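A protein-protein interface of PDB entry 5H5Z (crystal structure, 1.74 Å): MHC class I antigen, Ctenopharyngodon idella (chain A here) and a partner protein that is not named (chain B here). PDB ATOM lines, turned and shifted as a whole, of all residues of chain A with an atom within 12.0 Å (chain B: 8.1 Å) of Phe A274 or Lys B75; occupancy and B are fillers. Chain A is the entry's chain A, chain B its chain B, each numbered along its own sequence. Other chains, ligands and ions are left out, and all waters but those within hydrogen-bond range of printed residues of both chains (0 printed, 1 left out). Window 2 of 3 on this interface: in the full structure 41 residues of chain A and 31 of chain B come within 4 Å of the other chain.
The chain-end carboxylate (OXT) of Met B98 sits at hydrogen-bond distance from the side-chain hydroxyl (OG) of Ser B96 (2.9 Å).
NE2 of Gln A187 is in hydrogen-bond range of O of Pro A190 (3.3 Å).
The side-chain amide nitrogen (NE2) of Gln A187 lies close to the backbone carbonyl oxygen (O) of Asp A189, at 3.2 Å.
The backbone NH (N) of Glu B17 lies within hydrogen-bond range of the side-chain sulfur (SD) of Met B98 (3.6 Å).
O of Gln A187 sits at hydrogen-bond distance from OG1 of Thr A272, at 2.7 Å.
The backbone carbonyl oxygen of Ser A192 sits at hydrogen-bond distance from the side-chain amide nitrogen of Gln A187 (2.9 Å).
Among the printed residues, pairs that only touch across the chains: Leu A186 with Met B98 (3.8 Å), Gln A187 with Met B98 (3.6 Å), Ile A271 with Met B98 (3.9 Å), Asn A273 with Glu B17 (3.6 Å), Asn A273 with Ser B96 (3.97 Å) and Phe A274 with Lys B75 (3.4 Å).
The side-chain hydroxyl (OG1) of Thr A272 sits at hydrogen-bond distance from the chain-end carboxylate (O) of Met B98.
The side-chain amide oxygen of Asn A273 is in hydrogen-bond range of the backbone NH of Tyr B18 (3.1 Å).
The side-chain amino group of Lys A188 lies within salt-bridge range of the chain-end carboxylate of Met B98, at 2.9 Å.
N of Asn A273 is in hydrogen-bond range of O of Met B98 (2.9 Å).
OG of Ser B96 sits at hydrogen-bond distance from NZ of Lys A188 (3.3 Å).
Of the printed residues of chain B, Leu A186 touches Met B98.
Printed residues of chain B within 4 Å of Asn A273: Glu B17 (3.6 Å), Tyr B18 (3.1 Å), Ser B96 (3.97 Å) and Met B98 (2.9 Å).
Of the printed residues of chain A, Glu B17 touches Asn A273 (3.6 Å).
Of the printed residues of chain A, Tyr B18 touches Asn A273.
No residue of chain A comes within 4 Å of Glu B74.
Printed residues of chain A within 4 Å of Lys B75: Phe A274 (3.4 Å).
No residue of chain A comes within 4 Å of Asp B77.
Of the printed residues of chain A, Met B98 touches Leu A186 (3.8 Å), Gln A187 (3.6 Å), Lys A188 (2.9 Å), Ile A271 (3.9 Å), Thr A272 (3.2 Å) and Asn A273 (2.9 Å).
The nearest residue of chain B that does not touch Phe A274 is Tyr B18 (4.7 Å).
Of the 14 printed residues of chain B, 5 touch a printed residue of chain A.
Along chain A the printed residues that touch a printed residue of chain B span positions 186 to 274.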
ATOM      1  N   LEU A 186     -13.988 -16.494   7.035  1.00  0.00           N
ATOM      2  CA  LEU A 186     -13.199 -15.513   6.300  1.00  0.00           C
ATOM      3  C   LEU A 186     -13.803 -15.244   4.943  1.00  0.00           C
ATOM      4  O   LEU A 186     -14.333 -16.150   4.297  1.00  0.00           O
ATOM      5  CB  LEU A 186     -11.762 -16.017   6.115  1.00  0.00           C
ATOM      6  CG  LEU A 186     -11.013 -16.615   7.314  1.00  0.00           C
ATOM      7  CD1 LEU A 186      -9.610 -17.057   6.919  1.00  0.00           C
ATOM      8  CD2 LEU A 186     -10.970 -15.660   8.495  1.00  0.00           C
ATOM      9  N   GLN A 187     -13.721 -13.996   4.510  1.00  0.00           N
ATOM     10  CA  GLN A 187     -14.175 -13.627   3.178  1.00  0.00           C
ATOM     11  C   GLN A 187     -13.388 -12.425   2.685  1.00  0.00           C
ATOM     12  O   GLN A 187     -13.223 -11.447   3.410  1.00  0.00           O
ATOM     13  CB  GLN A 187     -15.667 -13.309   3.200  1.00  0.00           C
ATOM     14  CG  GLN A 187     -16.314 -13.319   1.828  1.00  0.00           C
ATOM     15  CD  GLN A 187     -17.796 -13.005   1.876  1.00  0.00           C
ATOM     16  OE1 GLN A 187     -18.252 -12.266   2.741  1.00  0.00           O
ATOM     17  NE2 GLN A 187     -18.552 -13.554   0.932  1.00  0.00           N
ATOM     18  N   LYS A 188     -12.900 -12.507   1.452  1.00  0.00           N
ATOM     19  CA  LYS A 188     -12.094 -11.437   0.876  1.00  0.00           C
ATOM     20  C   LYS A 188     -12.956 -10.297   0.341  1.00  0.00           C
ATOM     21  O   LYS A 188     -12.579  -9.131   0.422  1.00  0.00           O
ATOM     22  CB  LYS A 188     -11.195 -11.988  -0.228  1.00  0.00           C
ATOM     23  CG  LYS A 188     -10.180 -13.007   0.269  1.00  0.00           C
ATOM     24  CD  LYS A 188      -9.117 -13.309  -0.775  1.00  0.00           C
ATOM     25  CE  LYS A 188      -8.240 -12.098  -1.060  1.00  0.00           C
ATOM     26  NZ  LYS A 188      -7.102 -11.984  -0.108  1.00  0.00           N
ATOM     27  N   ASP A 189     -14.118 -10.649  -0.194  1.00  0.00           N
ATOM     28  CA  ASP A 189     -15.009  -9.699  -0.850  1.00  0.00           C
ATOM     29  C   ASP A 189     -16.430 -10.187  -0.603  1.00  0.00           C
ATOM     30  O   ASP A 189     -16.657 -11.395  -0.585  1.00  0.00           O
ATOM     31  CB  ASP A 189     -14.683  -9.674  -2.349  1.00  0.00           C
ATOM     32  CG  ASP A 189     -15.558  -8.725  -3.132  1.00  0.00           C
ATOM     33  OD1 ASP A 189     -16.707  -9.094  -3.444  1.00  0.00           O
ATOM     34  OD2 ASP A 189     -15.091  -7.611  -3.442  1.00  0.00           O
ATOM     35  N   PRO A 190     -17.396  -9.260  -0.408  1.00  0.00           N
ATOM     36  CA  PRO A 190     -18.775  -9.695  -0.145  1.00  0.00           C
ATOM     37  C   PRO A 190     -19.349 -10.647  -1.205  1.00  0.00           C
ATOM     38  O   PRO A 190     -20.288 -11.388  -0.916  1.00  0.00           O
ATOM     39  CB  PRO A 190     -19.559  -8.380  -0.133  1.00  0.00           C
ATOM     40  CG  PRO A 190     -18.565  -7.365   0.307  1.00  0.00           C
ATOM     41  CD  PRO A 190     -17.282  -7.786  -0.357  1.00  0.00           C
ATOM     42  N   SER A 192     -17.340 -12.870  -2.854  1.00  0.00           N
ATOM     43  CA  SER A 192     -16.365 -13.951  -2.977  1.00  0.00           C
ATOM     44  C   SER A 192     -16.730 -15.175  -2.133  1.00  0.00           C
ATOM     45  O   SER A 192     -17.659 -15.109  -1.322  1.00  0.00           O
ATOM     46  CB  SER A 192     -14.977 -13.434  -2.598  1.00  0.00           C
ATOM     47  OG  SER A 192     -14.481 -12.573  -3.603  1.00  0.00           O
ATOM     48  N   ILE A 270     -18.490 -13.303   9.948  1.00  0.00           N
ATOM     49  CA  ILE A 270     -17.550 -13.139   8.834  1.00  0.00           C
ATOM     50  C   ILE A 270     -16.606 -11.960   9.059  1.00  0.00           C
ATOM     51  O   ILE A 270     -17.041 -10.850   9.383  1.00  0.00           O
ATOM     52  CB  ILE A 270     -18.267 -13.035   7.464  1.00  0.00           C
ATOM     53  CG1 ILE A 270     -18.998 -14.347   7.155  1.00  0.00           C
ATOM     54  CG2 ILE A 270     -17.279 -12.693   6.348  1.00  0.00           C
ATOM     55  CD1 ILE A 270     -19.771 -14.350   5.855  1.00  0.00           C
ATOM     56  N   ILE A 271     -15.312 -12.230   8.913  1.00  0.00           N
ATOM     57  CA  ILE A 271     -14.292 -11.189   8.999  1.00  0.00           C
ATOM     58  C   ILE A 271     -13.576 -11.016   7.661  1.00  0.00           C
ATOM     59  O   ILE A 271     -13.554 -11.928   6.826  1.00  0.00           O
ATOM     60  CB  ILE A 271     -13.282 -11.426  10.153  1.00  0.00           C
ATOM     61  CG1 ILE A 271     -12.523 -12.751   9.976  1.00  0.00           C
ATOM     62  CG2 ILE A 271     -13.987 -11.343  11.504  1.00  0.00           C
ATOM     63  CD1 ILE A 271     -11.399 -12.954  10.973  1.00  0.00           C
ATOM     64  N   THR A 272     -13.003  -9.835   7.462  1.00  0.00           N
ATOM     65  CA  THR A 272     -12.341  -9.492   6.208  1.00  0.00           C
ATOM     66  C   THR A 272     -11.318  -8.384   6.436  1.00  0.00           C
ATOM     67  O   THR A 272     -11.409  -7.632   7.410  1.00  0.00           O
ATOM     68  CB  THR A 272     -13.373  -9.059   5.138  1.00  0.00           C
ATOM     69  OG1 THR A 272     -12.719  -8.829   3.880  1.00  0.00           O
ATOM     70  CG2 THR A 272     -14.118  -7.812   5.572  1.00  0.00           C
ATOM     71  N   ASN A 273     -10.331  -8.315   5.552  1.00  0.00           N
ATOM     72  CA  ASN A 273      -9.406  -7.193   5.496  1.00  0.00           C
ATOM     73  C   ASN A 273      -9.989  -6.121   4.579  1.00  0.00           C
ATOM     74  O   ASN A 273     -10.850  -6.425   3.749  1.00  0.00           O
ATOM     75  CB  ASN A 273      -8.043  -7.658   4.979  1.00  0.00           C
ATOM     76  CG  ASN A 273      -7.247  -8.426   6.022  1.00  0.00           C
ATOM     77  OD1 ASN A 273      -7.274  -8.103   7.210  1.00  0.00           O
ATOM     78  ND2 ASN A 273      -6.515  -9.439   5.577  1.00  0.00           N
ATOM     79  N   PHE A 274      -9.533  -4.876   4.727  1.00  0.00           N
ATOM     80  CA  PHE A 274     -10.092  -3.733   3.981  1.00  0.00           C
ATOM     81  C   PHE A 274     -11.534  -3.439   4.391  1.00  0.00           C
ATOM     82  O   PHE A 274     -11.915  -2.275   4.559  1.00  0.00           O
ATOM     83  CB  PHE A 274      -9.999  -3.944   2.458  1.00  0.00           C
ATOM     84  CG  PHE A 274      -9.176  -2.909   1.743  1.00  0.00           C
ATOM     85  CD1 PHE A 274      -7.956  -2.475   2.261  1.00  0.00           C
ATOM     86  CD2 PHE A 274      -9.627  -2.359   0.544  1.00  0.00           C
ATOM     87  CE1 PHE A 274      -7.204  -1.516   1.593  1.00  0.00           C
ATOM     88  CE2 PHE A 274      -8.877  -1.403  -0.126  1.00  0.00           C
ATOM     89  CZ  PHE A 274      -7.664  -0.980   0.400  1.00  0.00           C
ATOM     90  N   ASP A 275     -12.319  -4.508   4.537  1.00  0.00           N
ATOM     91  CA  ASP A 275     -13.699  -4.461   5.023  1.00  0.00           C
ATOM     92  C   ASP A 275     -14.640  -3.748   4.055  1.00  0.00           C
ATOM     93  O   ASP A 275     -15.843  -4.018   4.040  1.00  0.00           O
ATOM     94  CB  ASP A 275     -13.770  -3.817   6.408  1.00  0.00           C
ATOM     95  CG  ASP A 275     -12.897  -4.516   7.428  1.00  0.00           C
ATOM     96  OD1 ASP A 275     -13.366  -5.501   8.029  1.00  0.00           O
ATOM     97  OD2 ASP A 275     -11.750  -4.067   7.644  1.00  0.00           O
ATOM     98  N   GLU B  17      -5.257 -11.494   9.429  1.00  0.00           N
ATOM     99  CA  GLU B  17      -5.790 -10.163   9.703  1.00  0.00           C
ATOM    100  C   GLU B  17      -4.641  -9.160   9.759  1.00  0.00           C
ATOM    101  O   GLU B  17      -3.651  -9.391  10.455  1.00  0.00           O
ATOM    102  CB  GLU B  17      -6.549 -10.172  11.035  1.00  0.00           C
ATOM    103  CG  GLU B  17      -7.097  -8.822  11.472  1.00  0.00           C
ATOM    104  CD  GLU B  17      -7.597  -8.833  12.902  1.00  0.00           C
ATOM    105  OE1 GLU B  17      -7.354  -7.843  13.626  1.00  0.00           O
ATOM    106  OE2 GLU B  17      -8.229  -9.830  13.305  1.00  0.00           O
ATOM    107  N   TYR B  18      -4.774  -8.054   9.031  1.00  0.00           N
ATOM    108  CA  TYR B  18      -3.750  -7.007   9.027  1.00  0.00           C
ATOM    109  C   TYR B  18      -3.518  -6.397  10.401  1.00  0.00           C
ATOM    110  O   TYR B  18      -4.470  -6.125  11.142  1.00  0.00           O
ATOM    111  CB  TYR B  18      -4.106  -5.881   8.049  1.00  0.00           C
ATOM    112  CG  TYR B  18      -4.102  -6.274   6.591  1.00  0.00           C
ATOM    113  CD1 TYR B  18      -3.127  -7.130   6.072  1.00  0.00           C
ATOM    114  CD2 TYR B  18      -5.058  -5.759   5.721  1.00  0.00           C
ATOM    115  CE1 TYR B  18      -3.124  -7.479   4.732  1.00  0.00           C
ATOM    116  CE2 TYR B  18      -5.061  -6.104   4.381  1.00  0.00           C
ATOM    117  CZ  TYR B  18      -4.093  -6.960   3.893  1.00  0.00           C
ATOM    118  OH  TYR B  18      -4.100  -7.295   2.559  1.00  0.00           O
ATOM    119  N   GLY B  19      -2.246  -6.172  10.721  1.00  0.00           N
ATOM    120  CA  GLY B  19      -1.856  -5.537  11.978  1.00  0.00           C
ATOM    121  C   GLY B  19      -1.831  -6.462  13.183  1.00  0.00           C
ATOM    122  O   GLY B  19      -1.659  -6.002  14.309  1.00  0.00           O
ATOM    123  N   ASN B  43       8.341  -8.810   0.623  1.00  0.00           N
ATOM    124  CA  ASN B  43       8.575  -7.949  -0.539  1.00  0.00           C
ATOM    125  C   ASN B  43       9.810  -8.366  -1.354  1.00  0.00           C
ATOM    126  O   ASN B  43      10.591  -7.525  -1.804  1.00  0.00           O
ATOM    127  CB  ASN B  43       8.645  -6.474  -0.115  1.00  0.00           C
ATOM    128  CG  ASN B  43       7.386  -6.014   0.599  1.00  0.00           C
ATOM    129  OD1 ASN B  43       6.271  -6.363   0.205  1.00  0.00           O
ATOM    130  ND2 ASN B  43       7.557  -5.224   1.652  1.00  0.00           N
ATOM    131  N   LYS B  72       3.751  -9.852  10.858  1.00  0.00           N
ATOM    132  CA  LYS B  72       2.577  -9.037  11.090  1.00  0.00           C
ATOM    133  C   LYS B  72       2.161  -8.461   9.735  1.00  0.00           C
ATOM    134  O   LYS B  72       2.668  -7.416   9.325  1.00  0.00           O
ATOM    135  CB  LYS B  72       2.892  -7.934  12.105  1.00  0.00           C
ATOM    136  CG  LYS B  72       1.667  -7.211  12.649  1.00  0.00           C
ATOM    137  CD  LYS B  72       1.974  -6.440  13.925  1.00  0.00           C
ATOM    138  CE  LYS B  72       2.575  -5.076  13.631  1.00  0.00           C
ATOM    139  NZ  LYS B  72       2.556  -4.193  14.833  1.00  0.00           N
ATOM    140  N   PRO B  73       1.252  -9.161   9.023  1.00  0.00           N
ATOM    141  CA  PRO B  73       0.891  -8.722   7.671  1.00  0.00           C
ATOM    142  C   PRO B  73       0.189  -7.362   7.644  1.00  0.00           C
ATOM    143  O   PRO B  73      -0.696  -7.096   8.462  1.00  0.00           O
ATOM    144  CB  PRO B  73      -0.047  -9.828   7.174  1.00  0.00           C
ATOM    145  CG  PRO B  73      -0.597 -10.452   8.412  1.00  0.00           C
ATOM    146  CD  PRO B  73       0.512 -10.377   9.421  1.00  0.00           C
ATOM    147  N   GLU B  74       0.623  -6.506   6.726  1.00  0.00           N
ATOM    148  CA  GLU B  74       0.001  -5.199   6.506  1.00  0.00           C
ATOM    149  C   GLU B  74      -0.379  -5.073   5.033  1.00  0.00           C
ATOM    150  O   GLU B  74       0.075  -5.861   4.201  1.00  0.00           O
ATOM    151  CB  GLU B  74       0.939  -4.059   6.929  1.00  0.00           C
ATOM    152  CG  GLU B  74       1.434  -4.117   8.376  1.00  0.00           C
ATOM    153  CD  GLU B  74       0.384  -3.742   9.418  1.00  0.00           C
ATOM    154  OE1 GLU B  74      -0.760  -3.408   9.053  1.00  0.00           O
ATOM    155  OE2 GLU B  74       0.706  -3.781  10.625  1.00  0.00           O
ATOM    156  N   LYS B  75      -1.212  -4.083   4.720  1.00  0.00           N
ATOM    157  CA  LYS B  75      -1.747  -3.895   3.366  1.00  0.00           C
ATOM    158  C   LYS B  75      -0.715  -3.838   2.239  1.00  0.00           C
ATOM    159  O   LYS B  75      -0.908  -4.447   1.188  1.00  0.00           O
ATOM    160  CB  LYS B  75      -2.652  -2.658   3.302  1.00  0.00           C
ATOM    161  CG  LYS B  75      -4.103  -2.983   2.989  1.00  0.00           C
ATOM    162  CD  LYS B  75      -4.272  -3.399   1.532  1.00  0.00           C
ATOM    163  CE  LYS B  75      -5.380  -4.429   1.373  1.00  0.00           C
ATOM    164  NZ  LYS B  75      -5.890  -4.515  -0.027  1.00  0.00           N
ATOM    165  N   SER B  76       0.372  -3.107   2.461  1.00  0.00           N
ATOM    166  CA  SER B  76       1.337  -2.837   1.396  1.00  0.00           C
ATOM    167  C   SER B  76       2.459  -3.876   1.280  1.00  0.00           C
ATOM    168  O   SER B  76       3.370  -3.716   0.465  1.00  0.00           O
ATOM    169  CB  SER B  76       1.924  -1.429   1.555  1.00  0.00           C
ATOM    170  OG  SER B  76       2.598  -1.294   2.793  1.00  0.00           O
ATOM    171  N   ASP B  77       2.384  -4.941   2.078  1.00  0.00           N
ATOM    172  CA  ASP B  77       3.452  -5.947   2.118  1.00  0.00           C
ATOM    173  C   ASP B  77       3.057  -7.282   1.490  1.00  0.00           C
ATOM    174  O   ASP B  77       1.959  -7.790   1.726  1.00  0.00           O
ATOM    175  CB  ASP B  77       3.926  -6.167   3.558  1.00  0.00           C
ATOM    176  CG  ASP B  77       4.560  -4.928   4.161  1.00  0.00           C
ATOM    177  OD1 ASP B  77       5.364  -4.269   3.465  1.00  0.00           O
ATOM    178  OD2 ASP B  77       4.253  -4.614   5.333  1.00  0.00           O
ATOM    179  N   GLU B  78       3.970  -7.837   0.696  1.00  0.00           N
ATOM    180  CA  GLU B  78       3.793  -9.146   0.070  1.00  0.00           C
ATOM    181  C   GLU B  78       4.709 -10.185   0.709  1.00  0.00           C
ATOM    182  O   GLU B  78       5.908  -9.945   0.874  1.00  0.00           O
ATOM    183  CB  GLU B  78       4.077  -9.068  -1.434  1.00  0.00           C
ATOM    184  CG  GLU B  78       4.329 -10.424  -2.084  1.00  0.00           C
ATOM    185  CD  GLU B  78       5.062 -10.323  -3.407  1.00  0.00           C
ATOM    186  OE1 GLU B  78       4.425  -9.949  -4.407  1.00  0.00           O
ATOM    187  OE2 GLU B  78       6.271 -10.628  -3.450  1.00  0.00           O
ATOM    188  N   TYR B  79       4.137 -11.339   1.046  1.00  0.00           N
ATOM    189  CA  TYR B  79       4.902 -12.464   1.582  1.00  0.00           C
ATOM    190  C   TYR B  79       4.859 -13.650   0.637  1.00  0.00           C
ATOM    191  O   TYR B  79       3.856 -13.878  -0.047  1.00  0.00           O
ATOM    192  CB  TYR B  79       4.405 -12.843   2.979  1.00  0.00           C
ATOM    193  CG  TYR B  79       4.627 -11.729   3.975  1.00  0.00           C
ATOM    194  CD1 TYR B  79       3.657 -10.746   4.175  1.00  0.00           C
ATOM    195  CD2 TYR B  79       5.820 -11.636   4.694  1.00  0.00           C
ATOM    196  CE1 TYR B  79       3.866  -9.710   5.070  1.00  0.00           C
ATOM    197  CE2 TYR B  79       6.035 -10.605   5.592  1.00  0.00           C
ATOM    198  CZ  TYR B  79       5.054  -9.645   5.773  1.00  0.00           C
ATOM    199  OH  TYR B  79       5.262  -8.618   6.657  1.00  0.00           O
ATOM    200  N   SER B  96      -4.025 -14.517   1.867  1.00  0.00           N
ATOM    201  CA  SER B  96      -4.606 -14.343   3.204  1.00  0.00           C
ATOM    202  C   SER B  96      -6.002 -14.954   3.392  1.00  0.00           C
ATOM    203  O   SER B  96      -6.426 -15.187   4.521  1.00  0.00           O
ATOM    204  CB  SER B  96      -4.631 -12.862   3.593  1.00  0.00           C
ATOM    205  OG  SER B  96      -5.592 -12.160   2.839  1.00  0.00           O
ATOM    206  N   MET B  98      -8.488 -13.526   3.444  1.00  0.00           N
ATOM    207  CA  MET B  98      -9.230 -12.422   4.054  1.00  0.00           C
ATOM    208  C   MET B  98      -9.109 -11.151   3.234  1.00  0.00           C
ATOM    209  O   MET B  98      -9.854 -10.199   3.462  1.00  0.00           O
ATOM    210  CB  MET B  98      -8.680 -12.121   5.438  1.00  0.00           C
ATOM    211  CG  MET B  98      -9.268 -12.937   6.558  1.00  0.00           C
ATOM    212  SD  MET B  98      -8.516 -12.380   8.093  1.00  0.00           S
ATOM    213  CE  MET B  98      -9.399 -10.862   8.434  1.00  0.00           C
ATOM    214  OXT MET B  98      -8.255 -11.033   2.355  1.00  0.00           O
